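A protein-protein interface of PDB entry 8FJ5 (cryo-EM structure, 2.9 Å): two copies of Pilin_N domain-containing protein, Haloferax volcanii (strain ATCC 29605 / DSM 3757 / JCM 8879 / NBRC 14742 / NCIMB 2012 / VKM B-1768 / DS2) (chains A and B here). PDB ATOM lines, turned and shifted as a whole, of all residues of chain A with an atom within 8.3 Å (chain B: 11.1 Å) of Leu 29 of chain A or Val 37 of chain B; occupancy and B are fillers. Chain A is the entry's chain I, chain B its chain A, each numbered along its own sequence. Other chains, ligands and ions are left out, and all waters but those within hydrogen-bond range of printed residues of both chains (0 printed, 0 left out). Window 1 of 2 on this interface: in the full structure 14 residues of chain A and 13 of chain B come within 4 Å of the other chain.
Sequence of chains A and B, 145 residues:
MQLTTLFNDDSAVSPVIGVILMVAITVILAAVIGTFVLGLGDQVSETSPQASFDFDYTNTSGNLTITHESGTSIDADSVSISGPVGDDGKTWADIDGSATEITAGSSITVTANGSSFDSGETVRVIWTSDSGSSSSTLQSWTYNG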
ATOM      1  N   MET A  22     -26.012  -0.120 -24.419  1.00  0.00           N
ATOM      2  CA  MET A  22     -26.042   0.095 -22.975  1.00  0.00           C
ATOM      3  C   MET A  22     -24.657   0.427 -22.429  1.00  0.00           C
ATOM      4  O   MET A  22     -24.518   1.309 -21.572  1.00  0.00           O
ATOM      5  CB  MET A  22     -26.628  -1.130 -22.274  1.00  0.00           C
ATOM      6  CG  MET A  22     -28.097  -1.394 -22.597  1.00  0.00           C
ATOM      7  SD  MET A  22     -29.199  -0.059 -22.092  1.00  0.00           S
ATOM      8  CE  MET A  22     -29.512   0.766 -23.646  1.00  0.00           C
ATOM      9  N   VAL A  23     -23.620  -0.256 -22.916  1.00  0.00           N
ATOM     10  CA  VAL A  23     -22.258   0.054 -22.477  1.00  0.00           C
ATOM     11  C   VAL A  23     -21.868   1.466 -22.899  1.00  0.00           C
ATOM     12  O   VAL A  23     -21.224   2.212 -22.140  1.00  0.00           O
ATOM     13  CB  VAL A  23     -21.273  -0.998 -23.020  1.00  0.00           C
ATOM     14  CG1 VAL A  23     -19.841  -0.594 -22.735  1.00  0.00           C
ATOM     15  CG2 VAL A  23     -21.566  -2.356 -22.416  1.00  0.00           C
ATOM     16  N   ALA A  24     -22.247   1.854 -24.121  1.00  0.00           N
ATOM     17  CA  ALA A  24     -21.940   3.196 -24.603  1.00  0.00           C
ATOM     18  C   ALA A  24     -22.590   4.266 -23.733  1.00  0.00           C
ATOM     19  O   ALA A  24     -21.987   5.313 -23.472  1.00  0.00           O
ATOM     20  CB  ALA A  24     -22.383   3.341 -26.056  1.00  0.00           C
ATOM     21  N   ILE A  25     -23.829   4.033 -23.292  1.00  0.00           N
ATOM     22  CA  ILE A  25     -24.481   4.986 -22.391  1.00  0.00           C
ATOM     23  C   ILE A  25     -23.782   5.017 -21.035  1.00  0.00           C
ATOM     24  O   ILE A  25     -23.580   6.090 -20.440  1.00  0.00           O
ATOM     25  CB  ILE A  25     -25.976   4.647 -22.244  1.00  0.00           C
ATOM     26  CG1 ILE A  25     -26.700   4.803 -23.577  1.00  0.00           C
ATOM     27  CG2 ILE A  25     -26.624   5.540 -21.214  1.00  0.00           C
ATOM     28  CD1 ILE A  25     -28.109   4.265 -23.560  1.00  0.00           C
ATOM     29  N   THR A  26     -23.421   3.838 -20.516  1.00  0.00           N
ATOM     30  CA  THR A  26     -22.798   3.748 -19.199  1.00  0.00           C
ATOM     31  C   THR A  26     -21.503   4.541 -19.129  1.00  0.00           C
ATOM     32  O   THR A  26     -21.245   5.220 -18.127  1.00  0.00           O
ATOM     33  CB  THR A  26     -22.530   2.283 -18.847  1.00  0.00           C
ATOM     34  OG1 THR A  26     -23.772   1.586 -18.697  1.00  0.00           O
ATOM     35  CG2 THR A  26     -21.736   2.172 -17.562  1.00  0.00           C
ATOM     36  N   VAL A  27     -20.679   4.467 -20.175  1.00  0.00           N
ATOM     37  CA  VAL A  27     -19.382   5.145 -20.143  1.00  0.00           C
ATOM     38  C   VAL A  27     -19.566   6.657 -20.009  1.00  0.00           C
ATOM     39  O   VAL A  27     -18.928   7.313 -19.169  1.00  0.00           O
ATOM     40  CB  VAL A  27     -18.564   4.779 -21.393  1.00  0.00           C
ATOM     41  CG1 VAL A  27     -17.343   5.668 -21.511  1.00  0.00           C
ATOM     42  CG2 VAL A  27     -18.159   3.321 -21.343  1.00  0.00           C
ATOM     43  N   ILE A  28     -20.458   7.229 -20.822  1.00  0.00           N
ATOM     44  CA  ILE A  28     -20.695   8.670 -20.788  1.00  0.00           C
ATOM     45  C   ILE A  28     -21.251   9.092 -19.435  1.00  0.00           C
ATOM     46  O   ILE A  28     -20.819  10.097 -18.854  1.00  0.00           O
ATOM     47  CB  ILE A  28     -21.636   9.081 -21.937  1.00  0.00           C
ATOM     48  CG1 ILE A  28     -20.875   9.172 -23.255  1.00  0.00           C
ATOM     49  CG2 ILE A  28     -22.299  10.411 -21.645  1.00  0.00           C
ATOM     50  CD1 ILE A  28     -21.740   8.921 -24.455  1.00  0.00           C
ATOM     51  N   LEU A  29     -22.220   8.338 -18.912  1.00  0.00           N
ATOM     52  CA  LEU A  29     -22.843   8.743 -17.656  1.00  0.00           C
ATOM     53  C   LEU A  29     -21.839   8.681 -16.502  1.00  0.00           C
ATOM     54  O   LEU A  29     -21.833   9.554 -15.617  1.00  0.00           O
ATOM     55  CB  LEU A  29     -24.068   7.868 -17.397  1.00  0.00           C
ATOM     56  CG  LEU A  29     -25.119   8.319 -16.388  1.00  0.00           C
ATOM     57  CD1 LEU A  29     -25.755   9.613 -16.840  1.00  0.00           C
ATOM     58  CD2 LEU A  29     -26.171   7.244 -16.245  1.00  0.00           C
ATOM     59  N   ALA A  30     -20.959   7.676 -16.519  1.00  0.00           N
ATOM     60  CA  ALA A  30     -19.912   7.595 -15.509  1.00  0.00           C
ATOM     61  C   ALA A  30     -18.961   8.778 -15.595  1.00  0.00           C
ATOM     62  O   ALA A  30     -18.540   9.319 -14.565  1.00  0.00           O
ATOM     63  CB  ALA A  30     -19.144   6.284 -15.652  1.00  0.00           C
ATOM     64  N   ALA A  31     -18.593   9.188 -16.812  1.00  0.00           N
ATOM     65  CA  ALA A  31     -17.729  10.361 -16.950  1.00  0.00           C
ATOM     66  C   ALA A  31     -18.399  11.613 -16.393  1.00  0.00           C
ATOM     67  O   ALA A  31     -17.746  12.453 -15.749  1.00  0.00           O
ATOM     68  CB  ALA A  31     -17.347  10.562 -18.415  1.00  0.00           C
ATOM     69  N   VAL A  32     -19.704  11.753 -16.629  1.00  0.00           N
ATOM     70  CA  VAL A  32     -20.430  12.924 -16.136  1.00  0.00           C
ATOM     71  C   VAL A  32     -20.412  12.969 -14.609  1.00  0.00           C
ATOM     72  O   VAL A  32     -20.236  14.037 -14.012  1.00  0.00           O
ATOM     73  CB  VAL A  32     -21.865  12.950 -16.691  1.00  0.00           C
ATOM     74  CG1 VAL A  32     -22.603  14.171 -16.188  1.00  0.00           C
ATOM     75  CG2 VAL A  32     -21.832  12.975 -18.200  1.00  0.00           C
ATOM     76  N   ILE A  33     -20.606  11.823 -13.949  1.00  0.00           N
ATOM     77  CA  ILE A  33     -20.510  11.826 -12.483  1.00  0.00           C
ATOM     78  C   ILE A  33     -19.088  12.123 -12.026  1.00  0.00           C
ATOM     79  O   ILE A  33     -18.871  12.821 -11.025  1.00  0.00           O
ATOM     80  CB  ILE A  33     -20.997  10.504 -11.872  1.00  0.00           C
ATOM     81  CG1 ILE A  33     -22.460  10.270 -12.153  1.00  0.00           C
ATOM     82  CG2 ILE A  33     -20.789  10.491 -10.370  1.00  0.00           C
ATOM     83  CD1 ILE A  33     -22.816   8.912 -11.773  1.00  0.00           C
ATOM     84  N   GLY A  34     -18.101  11.529 -12.700  1.00  0.00           N
ATOM     85  CA  GLY A  34     -16.728  11.691 -12.264  1.00  0.00           C
ATOM     86  C   GLY A  34     -16.288  13.137 -12.252  1.00  0.00           C
ATOM     87  O   GLY A  34     -15.653  13.595 -11.298  1.00  0.00           O
ATOM     88  N   THR A  35     -16.639  13.881 -13.303  1.00  0.00           N
ATOM     89  CA  THR A  35     -16.277  15.297 -13.345  1.00  0.00           C
ATOM     90  C   THR A  35     -16.863  16.046 -12.154  1.00  0.00           C
ATOM     91  O   THR A  35     -16.169  16.825 -11.488  1.00  0.00           O
ATOM     92  CB  THR A  35     -16.748  15.919 -14.661  1.00  0.00           C
ATOM     93  OG1 THR A  35     -16.167  15.211 -15.759  1.00  0.00           O
ATOM     94  CG2 THR A  35     -16.341  17.377 -14.738  1.00  0.00           C
ATOM     95  N   PHE A  36     -18.140  15.796 -11.857  1.00  0.00           N
ATOM     96  CA  PHE A  36     -18.822  16.512 -10.784  1.00  0.00           C
ATOM     97  C   PHE A  36     -18.204  16.203  -9.426  1.00  0.00           C
ATOM     98  O   PHE A  36     -17.941  17.113  -8.631  1.00  0.00           O
ATOM     99  CB  PHE A  36     -20.309  16.153 -10.796  1.00  0.00           C
ATOM    100  CG  PHE A  36     -21.080  16.715  -9.638  1.00  0.00           C
ATOM    101  CD1 PHE A  36     -21.466  18.042  -9.624  1.00  0.00           C
ATOM    102  CD2 PHE A  36     -21.425  15.915  -8.567  1.00  0.00           C
ATOM    103  CE1 PHE A  36     -22.174  18.557  -8.561  1.00  0.00           C
ATOM    104  CE2 PHE A  36     -22.131  16.428  -7.503  1.00  0.00           C
ATOM    105  CZ  PHE A  36     -22.505  17.748  -7.500  1.00  0.00           C
ATOM    106  N   LEU B  29     -35.468   2.005 -29.071  1.00  0.00           N
ATOM    107  CA  LEU B  29     -35.706   1.828 -27.642  1.00  0.00           C
ATOM    108  C   LEU B  29     -34.478   2.238 -26.827  1.00  0.00           C
ATOM    109  O   LEU B  29     -34.602   2.846 -25.750  1.00  0.00           O
ATOM    110  CB  LEU B  29     -36.114   0.380 -27.376  1.00  0.00           C
ATOM    111  CG  LEU B  29     -36.798   0.018 -26.062  1.00  0.00           C
ATOM    112  CD1 LEU B  29     -38.122   0.737 -25.947  1.00  0.00           C
ATOM    113  CD2 LEU B  29     -37.010  -1.476 -26.002  1.00  0.00           C
ATOM    114  N   ALA B  30     -33.282   1.946 -27.348  1.00  0.00           N
ATOM    115  CA  ALA B  30     -32.060   2.380 -26.682  1.00  0.00           C
ATOM    116  C   ALA B  30     -31.961   3.898 -26.633  1.00  0.00           C
ATOM    117  O   ALA B  30     -31.541   4.465 -25.618  1.00  0.00           O
ATOM    118  CB  ALA B  30     -30.841   1.792 -27.384  1.00  0.00           C
ATOM    119  N   ALA B  31     -32.328   4.576 -27.724  1.00  0.00           N
ATOM    120  CA  ALA B  31     -32.310   6.039 -27.706  1.00  0.00           C
ATOM    121  C   ALA B  31     -33.273   6.594 -26.661  1.00  0.00           C
ATOM    122  O   ALA B  31     -32.966   7.580 -25.969  1.00  0.00           O
ATOM    123  CB  ALA B  31     -32.646   6.585 -29.092  1.00  0.00           C
ATOM    124  N   VAL B  32     -34.446   5.970 -26.532  1.00  0.00           N
ATOM    125  CA  VAL B  32     -35.434   6.433 -25.558  1.00  0.00           C
ATOM    126  C   VAL B  32     -34.891   6.312 -24.136  1.00  0.00           C
ATOM    127  O   VAL B  32     -35.088   7.207 -23.306  1.00  0.00           O
ATOM    128  CB  VAL B  32     -36.763   5.677 -25.729  1.00  0.00           C
ATOM    129  CG1 VAL B  32     -37.784   6.171 -24.727  1.00  0.00           C
ATOM    130  CG2 VAL B  32     -37.296   5.882 -27.126  1.00  0.00           C
ATOM    131  N   ILE B  33     -34.212   5.203 -23.820  1.00  0.00           N
ATOM    132  CA  ILE B  33     -33.609   5.101 -22.484  1.00  0.00           C
ATOM    133  C   ILE B  33     -32.491   6.120 -22.306  1.00  0.00           C
ATOM    134  O   ILE B  33     -32.319   6.696 -21.223  1.00  0.00           O
ATOM    135  CB  ILE B  33     -33.086   3.685 -22.197  1.00  0.00           C
ATOM    136  CG1 ILE B  33     -34.203   2.674 -22.185  1.00  0.00           C
ATOM    137  CG2 ILE B  33     -32.374   3.631 -20.859  1.00  0.00           C
ATOM    138  CD1 ILE B  33     -33.643   1.331 -22.152  1.00  0.00           C
ATOM    139  N   GLY B  34     -31.663   6.292 -23.337  1.00  0.00           N
ATOM    140  CA  GLY B  34     -30.521   7.177 -23.207  1.00  0.00           C
ATOM    141  C   GLY B  34     -30.920   8.595 -22.870  1.00  0.00           C
ATOM    142  O   GLY B  34     -30.317   9.230 -22.000  1.00  0.00           O
ATOM    143  N   THR B  35     -31.956   9.105 -23.539  1.00  0.00           N
ATOM    144  CA  THR B  35     -32.419  10.459 -23.243  1.00  0.00           C
ATOM    145  C   THR B  35     -32.829  10.587 -21.780  1.00  0.00           C
ATOM    146  O   THR B  35     -32.450  11.546 -21.094  1.00  0.00           O
ATOM    147  CB  THR B  35     -33.581  10.829 -24.165  1.00  0.00           C
ATOM    148  OG1 THR B  35     -33.163  10.721 -25.529  1.00  0.00           O
ATOM    149  CG2 THR B  35     -34.044  12.248 -23.899  1.00  0.00           C
ATOM    150  N   PHE B  36     -33.585   9.609 -21.280  1.00  0.00           N
ATOM    151  CA  PHE B  36     -34.096   9.667 -19.915  1.00  0.00           C
ATOM    152  C   PHE B  36     -32.965   9.630 -18.894  1.00  0.00           C
ATOM    153  O   PHE B  36     -32.941  10.427 -17.950  1.00  0.00           O
ATOM    154  CB  PHE B  36     -35.071   8.511 -19.684  1.00  0.00           C
ATOM    155  CG  PHE B  36     -35.540   8.385 -18.265  1.00  0.00           C
ATOM    156  CD1 PHE B  36     -36.518   9.225 -17.768  1.00  0.00           C
ATOM    157  CD2 PHE B  36     -35.009   7.422 -17.430  1.00  0.00           C
ATOM    158  CE1 PHE B  36     -36.949   9.108 -16.465  1.00  0.00           C
ATOM    159  CE2 PHE B  36     -35.436   7.305 -16.128  1.00  0.00           C
ATOM    160  CZ  PHE B  36     -36.407   8.148 -15.645  1.00  0.00           C
ATOM    161  N   VAL B  37     -32.015   8.707 -19.064  1.00  0.00           N
ATOM    162  CA  VAL B  37     -30.945   8.601 -18.074  1.00  0.00           C
ATOM    163  C   VAL B  37     -30.025   9.815 -18.129  1.00  0.00           C
ATOM    164  O   VAL B  37     -29.530  10.268 -17.090  1.00  0.00           O
ATOM    165  CB  VAL B  37     -30.160   7.283 -18.224  1.00  0.00           C
ATOM    166  CG1 VAL B  37     -31.071   6.095 -17.978  1.00  0.00           C
ATOM    167  CG2 VAL B  37     -29.501   7.185 -19.586  1.00  0.00           C
ATOM    168  N   LEU B  38     -29.779  10.371 -19.320  1.00  0.00           N
ATOM    169  CA  LEU B  38     -28.958  11.575 -19.401  1.00  0.00           C
ATOM    170  C   LEU B  38     -29.637  12.753 -18.714  1.00  0.00           C
ATOM    171  O   LEU B  38     -28.997  13.495 -17.956  1.00  0.00           O
ATOM    172  CB  LEU B  38     -28.658  11.897 -20.863  1.00  0.00           C
ATOM    173  CG  LEU B  38     -27.610  10.998 -21.516  1.00  0.00           C
ATOM    174  CD1 LEU B  38     -27.267  11.506 -22.894  1.00  0.00           C
ATOM    175  CD2 LEU B  38     -26.364  10.901 -20.653  1.00  0.00           C
ATOM    176  N   GLY B  39     -30.940  12.930 -18.949  1.00  0.00           N
ATOM    177  CA  GLY B  39     -31.663  13.981 -18.259  1.00  0.00           C
ATOM    178  C   GLY B  39     -31.693  13.792 -16.757  1.00  0.00           C
ATOM    179  O   GLY B  39     -31.629  14.765 -16.004  1.00  0.00           O
ATOM    180  N   LEU B  40     -31.805  12.546 -16.300  1.00  0.00           N
ATOM    181  CA  LEU B  40     -31.765  12.265 -14.869  1.00  0.00           C
ATOM    182  C   LEU B  40     -30.403  12.604 -14.275  1.00  0.00           C
ATOM    183  O   LEU B  40     -30.323  13.151 -13.171  1.00  0.00           O
ATOM    184  CB  LEU B  40     -32.118  10.796 -14.624  1.00  0.00           C
ATOM    185  CG  LEU B  40     -32.477  10.283 -13.231  1.00  0.00           C
ATOM    186  CD1 LEU B  40     -33.263   8.996 -13.369  1.00  0.00           C
ATOM    187  CD2 LEU B  40     -31.249  10.050 -12.370  1.00  0.00           C
ATOM    188  N   GLY B  41     -29.324  12.285 -14.991  1.00  0.00           N
ATOM    189  CA  GLY B  41     -27.992  12.578 -14.498  1.00  0.00           C
ATOM    190  C   GLY B  41     -27.616  14.043 -14.545  1.00  0.00           C
ATOM    191  O   GLY B  41     -26.717  14.463 -13.810  1.00  0.00           O
ATOM    192  N   ASP B  42     -28.276  14.835 -15.394  1.00  0.00           N
ATOM    193  CA  ASP B  42     -27.964  16.260 -15.450  1.00  0.00           C
ATOM    194  C   ASP B  42     -28.549  17.043 -14.278  1.00  0.00           C
ATOM    195  O   ASP B  42     -28.168  18.200 -14.067  1.00  0.00           O
ATOM    196  CB  ASP B  42     -28.464  16.866 -16.761  1.00  0.00           C
ATOM    197  CG  ASP B  42     -27.802  18.196 -17.079  1.00  0.00           C
ATOM    198  OD1 ASP B  42     -26.574  18.313 -16.889  1.00  0.00           O
ATOM    199  OD2 ASP B  42     -28.514  19.129 -17.505  1.00  0.00           O
ATOM    200  N   GLN B  43     -29.460  16.450 -13.512  1.00  0.00           N
ATOM    201  CA  GLN B  43     -30.225  17.203 -12.523  1.00  0.00           C
ATOM    202  C   GLN B  43     -29.428  17.601 -11.284  1.00  0.00           C
ATOM    203  O   GLN B  43     -29.775  18.585 -10.624  1.00  0.00           O
ATOM    204  CB  GLN B  43     -31.456  16.404 -12.092  1.00  0.00           C
ATOM    205  CG  GLN B  43     -32.545  16.318 -13.146  1.00  0.00           C
ATOM    206  CD  GLN B  43     -33.718  15.471 -12.697  1.00  0.00           C
ATOM    207  OE1 GLN B  43     -33.705  14.904 -11.606  1.00  0.00           O
ATOM    208  NE2 GLN B  43     -34.738  15.377 -13.540  1.00  0.00           N
ATOM    209  N   VAL B  44     -28.366  16.869 -10.953  1.00  0.00           N
ATOM    210  CA  VAL B  44     -27.666  17.061  -9.682  1.00  0.00           C
ATOM    211  C   VAL B  44     -26.536  18.069  -9.882  1.00  0.00           C
ATOM    212  O   VAL B  44     -25.666  17.875 -10.738  1.00  0.00           O
ATOM    213  CB  VAL B  44     -27.136  15.740  -9.093  1.00  0.00           C
ATOM    214  CG1 VAL B  44     -26.086  15.088  -9.990  1.00  0.00           C
ATOM    215  CG2 VAL B  44     -26.575  15.976  -7.701  1.00  0.00           C
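Gly 34 of chain B touches Ile 25 of chain A.
CG2 of Val 37 of chain B touches CG2 of Ile 25 of chain A, at 3.7 Å.
Val 37 of chain B touches Leu 29 of chain A (O to CD1, 3.8 Å).
Printed residues of chain B within 4 Å of Ile 25 of chain A: Gly 34 (3.8 Å) and Val 37 (3.7 Å).
No residue of chain B comes within 4 Å of Val 27 of chain A.
No residue of chain B comes within 4 Å of Ile 28 of chain A.
Leu 29 of chain A touches just one residue of chain B: Val 37 (3.8 Å).
No residue of chain B comes within 4 Å of Ala 30 of chain A.
No residue of chain B comes within 4 Å of Ala 31 of chain A.
No residue of chain B comes within 4 Å of Ile 33 of chain A.
Printed residues of chain A within 4 Å of Gly 34 of chain B: Ile 25.
The nearest residue of chain B that does not touch Leu 29 of chain A is Leu 38 of chain B (4.1 Å).
The nearest residue of chain A that does not touch Val 37 of chain B is Thr 26 of chain A (7.0 Å).
The nearest printed residue of chain A that does not touch Gly 34 of chain B is Met 22 of chain A (5.9 Å).
Of the 16 printed residues of chain B, 2 touch a printed residue of chain A.
Hydrophobic or aromatic side chains of chain B that line the printed part of chain A: Val 37.
Among the printed residues, 3 pairs touch across the chains.
Among the printed residues, no Asp or Glu carboxylate lies within 4 Å of a Lys or Arg side-chain nitrogen of the other chain.
Positions printed for both chains: 29, 30, 31, 32, 33, 34, 35 and 36.
Of the 3 pairs that touch across the chains among the printed residues, none has its exchanged pair printed and touching as well.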
